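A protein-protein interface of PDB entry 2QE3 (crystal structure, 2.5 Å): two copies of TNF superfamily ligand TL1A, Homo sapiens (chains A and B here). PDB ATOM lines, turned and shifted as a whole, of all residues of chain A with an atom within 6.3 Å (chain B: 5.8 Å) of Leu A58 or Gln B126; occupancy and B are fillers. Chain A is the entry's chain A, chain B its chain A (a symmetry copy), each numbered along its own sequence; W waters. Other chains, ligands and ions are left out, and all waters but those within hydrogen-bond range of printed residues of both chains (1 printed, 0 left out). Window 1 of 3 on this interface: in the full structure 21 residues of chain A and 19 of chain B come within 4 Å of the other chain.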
ATOM      1  N   HIS A  31      -0.934  16.125 -31.802  1.00  0.00           N
ATOM      2  CA  HIS A  31      -0.862  17.035 -30.671  1.00  0.00           C
ATOM      3  C   HIS A  31       0.534  17.330 -30.207  1.00  0.00           C
ATOM      4  O   HIS A  31       1.203  16.439 -29.722  1.00  0.00           O
ATOM      5  CB  HIS A  31      -1.590  16.438 -29.513  1.00  0.00           C
ATOM      6  CG  HIS A  31      -1.728  17.383 -28.394  1.00  0.00           C
ATOM      7  ND1 HIS A  31      -2.561  18.476 -28.461  1.00  0.00           N
ATOM      8  CD2 HIS A  31      -1.135  17.424 -27.184  1.00  0.00           C
ATOM      9  CE1 HIS A  31      -2.457  19.163 -27.339  1.00  0.00           C
ATOM     10  NE2 HIS A  31      -1.604  18.540 -26.545  1.00  0.00           N
ATOM     11  N   LEU A  32       0.987  18.567 -30.333  1.00  0.00           N
ATOM     12  CA  LEU A  32       2.376  18.851 -29.973  1.00  0.00           C
ATOM     13  C   LEU A  32       2.485  19.708 -28.749  1.00  0.00           C
ATOM     14  O   LEU A  32       1.672  20.598 -28.530  1.00  0.00           O
ATOM     15  CB  LEU A  32       3.066  19.626 -31.064  1.00  0.00           C
ATOM     16  CG  LEU A  32       2.974  19.008 -32.417  1.00  0.00           C
ATOM     17  CD1 LEU A  32       3.851  19.762 -33.417  1.00  0.00           C
ATOM     18  CD2 LEU A  32       3.516  17.645 -32.197  1.00  0.00           C
ATOM     19  N   THR A  33       3.568  19.520 -28.010  1.00  0.00           N
ATOM     20  CA  THR A  33       3.712  20.229 -26.758  1.00  0.00           C
ATOM     21  C   THR A  33       5.021  20.989 -26.657  1.00  0.00           C
ATOM     22  O   THR A  33       5.933  20.690 -27.379  1.00  0.00           O
ATOM     23  CB  THR A  33       3.643  19.265 -25.576  1.00  0.00           C
ATOM     24  OG1 THR A  33       4.622  18.228 -25.716  1.00  0.00           O
ATOM     25  CG2 THR A  33       2.264  18.656 -25.434  1.00  0.00           C
ATOM     26  N   GLU A  55       6.591  13.340 -29.530  1.00  0.00           N
ATOM     27  CA  GLU A  55       6.462  11.894 -29.268  1.00  0.00           C
ATOM     28  C   GLU A  55       6.518  11.545 -27.788  1.00  0.00           C
ATOM     29  O   GLU A  55       5.922  10.591 -27.349  1.00  0.00           O
ATOM     30  CB  GLU A  55       7.540  11.091 -29.969  1.00  0.00           C
ATOM     31  CG  GLU A  55       8.939  11.700 -29.763  1.00  0.00           C
ATOM     32  CD  GLU A  55      10.103  10.822 -30.286  1.00  0.00           C
ATOM     33  OE1 GLU A  55       9.872   9.702 -30.877  1.00  0.00           O
ATOM     34  OE2 GLU A  55      11.256  11.283 -30.061  1.00  0.00           O
ATOM     35  N   LEU A  56       7.221  12.333 -27.025  1.00  0.00           N
ATOM     36  CA  LEU A  56       7.353  12.104 -25.618  1.00  0.00           C
ATOM     37  C   LEU A  56       6.176  12.690 -24.863  1.00  0.00           C
ATOM     38  O   LEU A  56       5.513  13.595 -25.359  1.00  0.00           O
ATOM     39  CB  LEU A  56       8.657  12.749 -25.153  1.00  0.00           C
ATOM     40  CG  LEU A  56       9.966  12.223 -25.752  1.00  0.00           C
ATOM     41  CD1 LEU A  56      11.045  13.295 -25.610  1.00  0.00           C
ATOM     42  CD2 LEU A  56      10.426  10.932 -25.061  1.00  0.00           C
ATOM     43  N   GLY A  57       5.946  12.194 -23.644  1.00  0.00           N
ATOM     44  CA  GLY A  57       4.818  12.620 -22.804  1.00  0.00           C
ATOM     45  C   GLY A  57       3.479  12.456 -23.497  1.00  0.00           C
ATOM     46  O   GLY A  57       3.163  11.380 -23.997  1.00  0.00           O
ATOM     47  N   LEU A  58       2.726  13.552 -23.590  1.00  0.00           N
ATOM     48  CA  LEU A  58       1.435  13.501 -24.251  1.00  0.00           C
ATOM     49  C   LEU A  58       1.468  13.830 -25.716  1.00  0.00           C
ATOM     50  O   LEU A  58       0.413  13.768 -26.344  1.00  0.00           O
ATOM     51  CB  LEU A  58       0.466  14.499 -23.629  1.00  0.00           C
ATOM     52  CG  LEU A  58       0.158  14.351 -22.160  1.00  0.00           C
ATOM     53  CD1 LEU A  58      -0.690  15.569 -21.675  1.00  0.00           C
ATOM     54  CD2 LEU A  58      -0.469  12.963 -21.823  1.00  0.00           C
ATOM     55  N   ALA A  59       2.600  14.248 -26.279  1.00  0.00           N
ATOM     56  CA  ALA A  59       2.546  14.632 -27.708  1.00  0.00           C
ATOM     57  C   ALA A  59       2.527  13.423 -28.609  1.00  0.00           C
ATOM     58  O   ALA A  59       2.933  12.317 -28.213  1.00  0.00           O
ATOM     59  CB  ALA A  59       3.693  15.573 -28.110  1.00  0.00           C
ATOM     60  N   PHE A  60       2.092  13.632 -29.838  1.00  0.00           N
ATOM     61  CA  PHE A  60       2.146  12.520 -30.746  1.00  0.00           C
ATOM     62  C   PHE A  60       1.845  13.024 -32.135  1.00  0.00           C
ATOM     63  O   PHE A  60       1.192  14.056 -32.333  1.00  0.00           O
ATOM     64  CB  PHE A  60       1.085  11.518 -30.337  1.00  0.00           C
ATOM     65  CG  PHE A  60      -0.345  11.979 -30.670  1.00  0.00           C
ATOM     66  CD1 PHE A  60      -0.823  11.961 -31.963  1.00  0.00           C
ATOM     67  CD2 PHE A  60      -1.202  12.452 -29.670  1.00  0.00           C
ATOM     68  CE1 PHE A  60      -2.103  12.435 -32.251  1.00  0.00           C
ATOM     69  CE2 PHE A  60      -2.499  12.893 -29.949  1.00  0.00           C
ATOM     70  CZ  PHE A  60      -2.944  12.887 -31.231  1.00  0.00           C
ATOM     71  N   GLU A 174       4.050  20.694 -20.153  1.00  0.00           N
ATOM     72  CA  GLU A 174       3.452  20.361 -21.453  1.00  0.00           C
ATOM     73  C   GLU A 174       2.018  20.728 -21.563  1.00  0.00           C
ATOM     74  O   GLU A 174       1.444  20.550 -22.635  1.00  0.00           O
ATOM     75  CB  GLU A 174       3.522  18.861 -21.802  1.00  0.00           C
ATOM     76  CG  GLU A 174       2.861  17.850 -20.797  1.00  0.00           C
ATOM     77  CD  GLU A 174       2.947  16.335 -21.227  1.00  0.00           C
ATOM     78  OE1 GLU A 174       3.250  16.052 -22.439  1.00  0.00           O
ATOM     79  OE2 GLU A 174       2.692  15.433 -20.355  1.00  0.00           O
ATOM     80  N   ASP A 175       1.391  21.196 -20.490  1.00  0.00           N
ATOM     81  CA  ASP A 175      -0.032  21.381 -20.614  1.00  0.00           C
ATOM     82  C   ASP A 175      -0.333  22.815 -20.615  1.00  0.00           C
ATOM     83  O   ASP A 175      -1.482  23.164 -20.447  1.00  0.00           O
ATOM     84  CB  ASP A 175      -0.815  20.675 -19.509  1.00  0.00           C
ATOM     85  CG  ASP A 175      -0.358  21.069 -18.133  1.00  0.00           C
ATOM     86  OD1 ASP A 175       0.641  21.824 -17.968  1.00  0.00           O
ATOM     87  OD2 ASP A 175      -1.012  20.595 -17.198  1.00  0.00           O
ATOM     88  N   VAL B 113      -7.291  23.249 -14.534  1.00  0.00           N
ATOM     89  CA  VAL B 113      -6.728  22.049 -15.081  1.00  0.00           C
ATOM     90  C   VAL B 113      -7.739  20.978 -15.414  1.00  0.00           C
ATOM     91  O   VAL B 113      -8.631  20.647 -14.638  1.00  0.00           O
ATOM     92  CB  VAL B 113      -5.844  21.420 -14.095  1.00  0.00           C
ATOM     93  CG1 VAL B 113      -4.951  20.423 -14.770  1.00  0.00           C
ATOM     94  CG2 VAL B 113      -5.005  22.438 -13.528  1.00  0.00           C
ATOM     95  N   ILE B 114      -7.563  20.402 -16.573  1.00  0.00           N
ATOM     96  CA  ILE B 114      -8.334  19.266 -16.966  1.00  0.00           C
ATOM     97  C   ILE B 114      -7.422  18.149 -16.869  1.00  0.00           C
ATOM     98  O   ILE B 114      -6.361  18.197 -17.433  1.00  0.00           O
ATOM     99  CB  ILE B 114      -8.704  19.320 -18.408  1.00  0.00           C
ATOM    100  CG1 ILE B 114      -9.023  20.762 -18.826  1.00  0.00           C
ATOM    101  CG2 ILE B 114      -9.836  18.476 -18.641  1.00  0.00           C
ATOM    102  CD1 ILE B 114     -10.295  20.904 -19.643  1.00  0.00           C
ATOM    103  N   THR B 115      -7.907  17.102 -16.243  1.00  0.00           N
ATOM    104  CA  THR B 115      -7.075  16.108 -15.659  1.00  0.00           C
ATOM    105  C   THR B 115      -7.581  14.711 -15.822  1.00  0.00           C
ATOM    106  O   THR B 115      -8.788  14.376 -15.646  1.00  0.00           O
ATOM    107  CB  THR B 115      -6.960  16.412 -14.212  1.00  0.00           C
ATOM    108  OG1 THR B 115      -5.694  17.035 -14.038  1.00  0.00           O
ATOM    109  CG2 THR B 115      -6.938  15.200 -13.433  1.00  0.00           C
ATOM    110  N   LYS B 116      -6.633  13.869 -16.149  1.00  0.00           N
ATOM    111  CA  LYS B 116      -6.983  12.508 -16.497  1.00  0.00           C
ATOM    112  C   LYS B 116      -6.575  11.631 -15.387  1.00  0.00           C
ATOM    113  O   LYS B 116      -5.472  11.763 -14.847  1.00  0.00           O
ATOM    114  CB  LYS B 116      -6.248  12.038 -17.752  1.00  0.00           C
ATOM    115  CG  LYS B 116      -6.295  10.540 -17.967  1.00  0.00           C
ATOM    116  CD  LYS B 116      -5.637  10.155 -19.328  1.00  0.00           C
ATOM    117  CE  LYS B 116      -4.129   9.733 -19.244  1.00  0.00           C
ATOM    118  NZ  LYS B 116      -3.339   9.836 -20.553  1.00  0.00           N
ATOM    119  N   PRO B 124      -2.385  10.998 -11.014  1.00  0.00           N
ATOM    120  CA  PRO B 124      -3.294  11.600 -11.938  1.00  0.00           C
ATOM    121  C   PRO B 124      -2.452  12.428 -12.866  1.00  0.00           C
ATOM    122  O   PRO B 124      -1.369  12.824 -12.511  1.00  0.00           O
ATOM    123  CB  PRO B 124      -4.111  12.508 -11.047  1.00  0.00           C
ATOM    124  CG  PRO B 124      -3.161  12.980 -10.045  1.00  0.00           C
ATOM    125  CD  PRO B 124      -2.222  11.818  -9.802  1.00  0.00           C
ATOM    126  N   THR B 125      -2.967  12.717 -14.045  1.00  0.00           N
ATOM    127  CA  THR B 125      -2.168  13.214 -15.146  1.00  0.00           C
ATOM    128  C   THR B 125      -2.840  14.495 -15.646  1.00  0.00           C
ATOM    129  O   THR B 125      -4.088  14.572 -15.755  1.00  0.00           O
ATOM    130  CB  THR B 125      -2.161  12.133 -16.237  1.00  0.00           C
ATOM    131  OG1 THR B 125      -1.817  10.825 -15.678  1.00  0.00           O
ATOM    132  CG2 THR B 125      -1.250  12.504 -17.339  1.00  0.00           C
ATOM    133  N   GLN B 126      -2.030  15.512 -15.901  1.00  0.00           N
ATOM    134  CA  GLN B 126      -2.559  16.815 -16.229  1.00  0.00           C
ATOM    135  C   GLN B 126      -2.478  17.066 -17.708  1.00  0.00           C
ATOM    136  O   GLN B 126      -1.377  17.195 -18.288  1.00  0.00           O
ATOM    137  CB  GLN B 126      -1.776  17.935 -15.544  1.00  0.00           C
ATOM    138  CG  GLN B 126      -2.067  18.121 -14.096  1.00  0.00           C
ATOM    139  CD  GLN B 126      -1.213  19.203 -13.450  1.00  0.00           C
ATOM    140  OE1 GLN B 126      -0.597  19.002 -12.375  1.00  0.00           O
ATOM    141  NE2 GLN B 126      -1.182  20.362 -14.085  1.00  0.00           N
ATOM    142  N   LEU B 127      -3.651  17.203 -18.304  1.00  0.00           N
ATOM    143  CA  LEU B 127      -3.721  17.443 -19.696  1.00  0.00           C
ATOM    144  C   LEU B 127      -3.736  18.874 -20.082  1.00  0.00           C
ATOM    145  O   LEU B 127      -3.184  19.200 -21.086  1.00  0.00           O
ATOM    146  CB  LEU B 127      -4.999  16.917 -20.197  1.00  0.00           C
ATOM    147  CG  LEU B 127      -5.194  15.459 -19.848  1.00  0.00           C
ATOM    148  CD1 LEU B 127      -6.491  14.893 -20.407  1.00  0.00           C
ATOM    149  CD2 LEU B 127      -4.114  14.734 -20.442  1.00  0.00           C
ATOM    150  N   LEU B 128      -4.474  19.730 -19.396  1.00  0.00           N
ATOM    151  CA  LEU B 128      -4.588  21.062 -19.958  1.00  0.00           C
ATOM    152  C   LEU B 128      -4.525  21.934 -18.773  1.00  0.00           C
ATOM    153  O   LEU B 128      -5.234  21.686 -17.765  1.00  0.00           O
ATOM    154  CB  LEU B 128      -5.916  21.265 -20.697  1.00  0.00           C
ATOM    155  CG  LEU B 128      -6.078  20.456 -21.976  1.00  0.00           C
ATOM    156  CD1 LEU B 128      -7.288  20.795 -22.815  1.00  0.00           C
ATOM    157  CD2 LEU B 128      -4.918  20.874 -22.726  1.00  0.00           C
ATOM    158  N   MET B 129      -3.671  22.951 -18.854  1.00  0.00           N
ATOM    159  CA  MET B 129      -3.747  23.987 -17.826  1.00  0.00           C
ATOM    160  C   MET B 129      -3.807  25.407 -18.287  1.00  0.00           C
ATOM    161  O   MET B 129      -2.849  25.965 -18.857  1.00  0.00           O
ATOM    162  CB  MET B 129      -2.617  23.842 -16.869  1.00  0.00           C
ATOM    163  CG  MET B 129      -2.499  25.000 -15.926  1.00  0.00           C
ATOM    164  SD  MET B 129      -0.862  25.045 -15.075  1.00  0.00           S
ATOM    165  CE  MET B 129      -1.228  24.036 -13.629  1.00  0.00           C
ATOM    166  N   PHE B 151      -6.698  14.374 -27.217  1.00  0.00           N
ATOM    167  CA  PHE B 151      -5.901  13.411 -26.496  1.00  0.00           C
ATOM    168  C   PHE B 151      -6.324  12.024 -26.799  1.00  0.00           C
ATOM    169  O   PHE B 151      -7.524  11.752 -27.106  1.00  0.00           O
ATOM    170  CB  PHE B 151      -5.934  13.614 -25.002  1.00  0.00           C
ATOM    171  CG  PHE B 151      -5.600  14.999 -24.595  1.00  0.00           C
ATOM    172  CD1 PHE B 151      -4.287  15.359 -24.324  1.00  0.00           C
ATOM    173  CD2 PHE B 151      -6.589  15.979 -24.506  1.00  0.00           C
ATOM    174  CE1 PHE B 151      -3.965  16.679 -23.923  1.00  0.00           C
ATOM    175  CE2 PHE B 151      -6.269  17.298 -24.110  1.00  0.00           C
ATOM    176  CZ  PHE B 151      -4.953  17.628 -23.817  1.00  0.00           C
HETATM  177  O   HOH W   1      -1.291  18.907 -23.120  1.00  0.00           O
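Of the 11 printed residues of chain B, 5 touch a printed residue of chain A.
Among the printed residues, no Asp or Glu carboxylate lies within 4 Å of a Lys or Arg side-chain nitrogen of the other chain.
The backbone NH of Met B129 sits at hydrogen-bond distance from the backbone carbonyl oxygen of Asp A175 (2.7 Å).
The side-chain carboxylate (OD2) of Asp A175 lies within hydrogen-bond range of the side-chain amide nitrogen (NE2) of Gln B126.
Of chain B, only Gln B126 and Leu B127 come within 4 Å of Leu A58.
Gln B126 touches two residues of chain A.
Printed residues of chain A within 4 Å of Leu B128: Asp A175.
Printed residues of chain B within 4 Å of Asp A175: Gln B126, Leu B127, Leu B128 and Met B129.
Printed residues of chain B within 4 Å of His A31: Phe B151.
Printed residues of chain A within 4 Å of Phe B151: His A31.
Of the printed residues of chain A, Met B129 touches Asp A175 (2.7 Å).
No position is printed for both chains.
Of the 7 pairs that touch across the chains among the printed residues, none has its exchanged pair printed and touching as well.
Water W1 lies within hydrogen-bond range of the backbone carbonyl oxygen (O) of Leu B127 (2.8 Å), the backbone carbonyl oxygen (O) of Glu A174 (3.2 Å) and a ring nitrogen (NE2) of His A31 (3.5 Å).
The backbone NH (N) of Ile B114 lies within hydrogen-bond range of the backbone carbonyl oxygen (O) of Leu B128 (2.9 Å).
The backbone carbonyl oxygen of Ile B114 sits at hydrogen-bond distance from the backbone NH of Leu B127 (3.0 Å).
The side-chain carboxylate (OE1) of Glu A174 is in hydrogen-bond range of the backbone NH (N) of Leu A58 (2.8 Å).
The backbone carbonyl oxygen of His A31 is in hydrogen-bond range of the backbone NH of Phe A60 (2.9 Å).
Among the printed residues, pairs that only touch across the chains: Asp A175 with Leu B127 (3.2 Å), Asp A175 with Leu B128 (3.7 Å), Leu A58 with Leu B127 (3.7 Å), Leu A58 with Gln B126 (3.8 Å) and His A31 with Phe B151 (3.99 Å).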
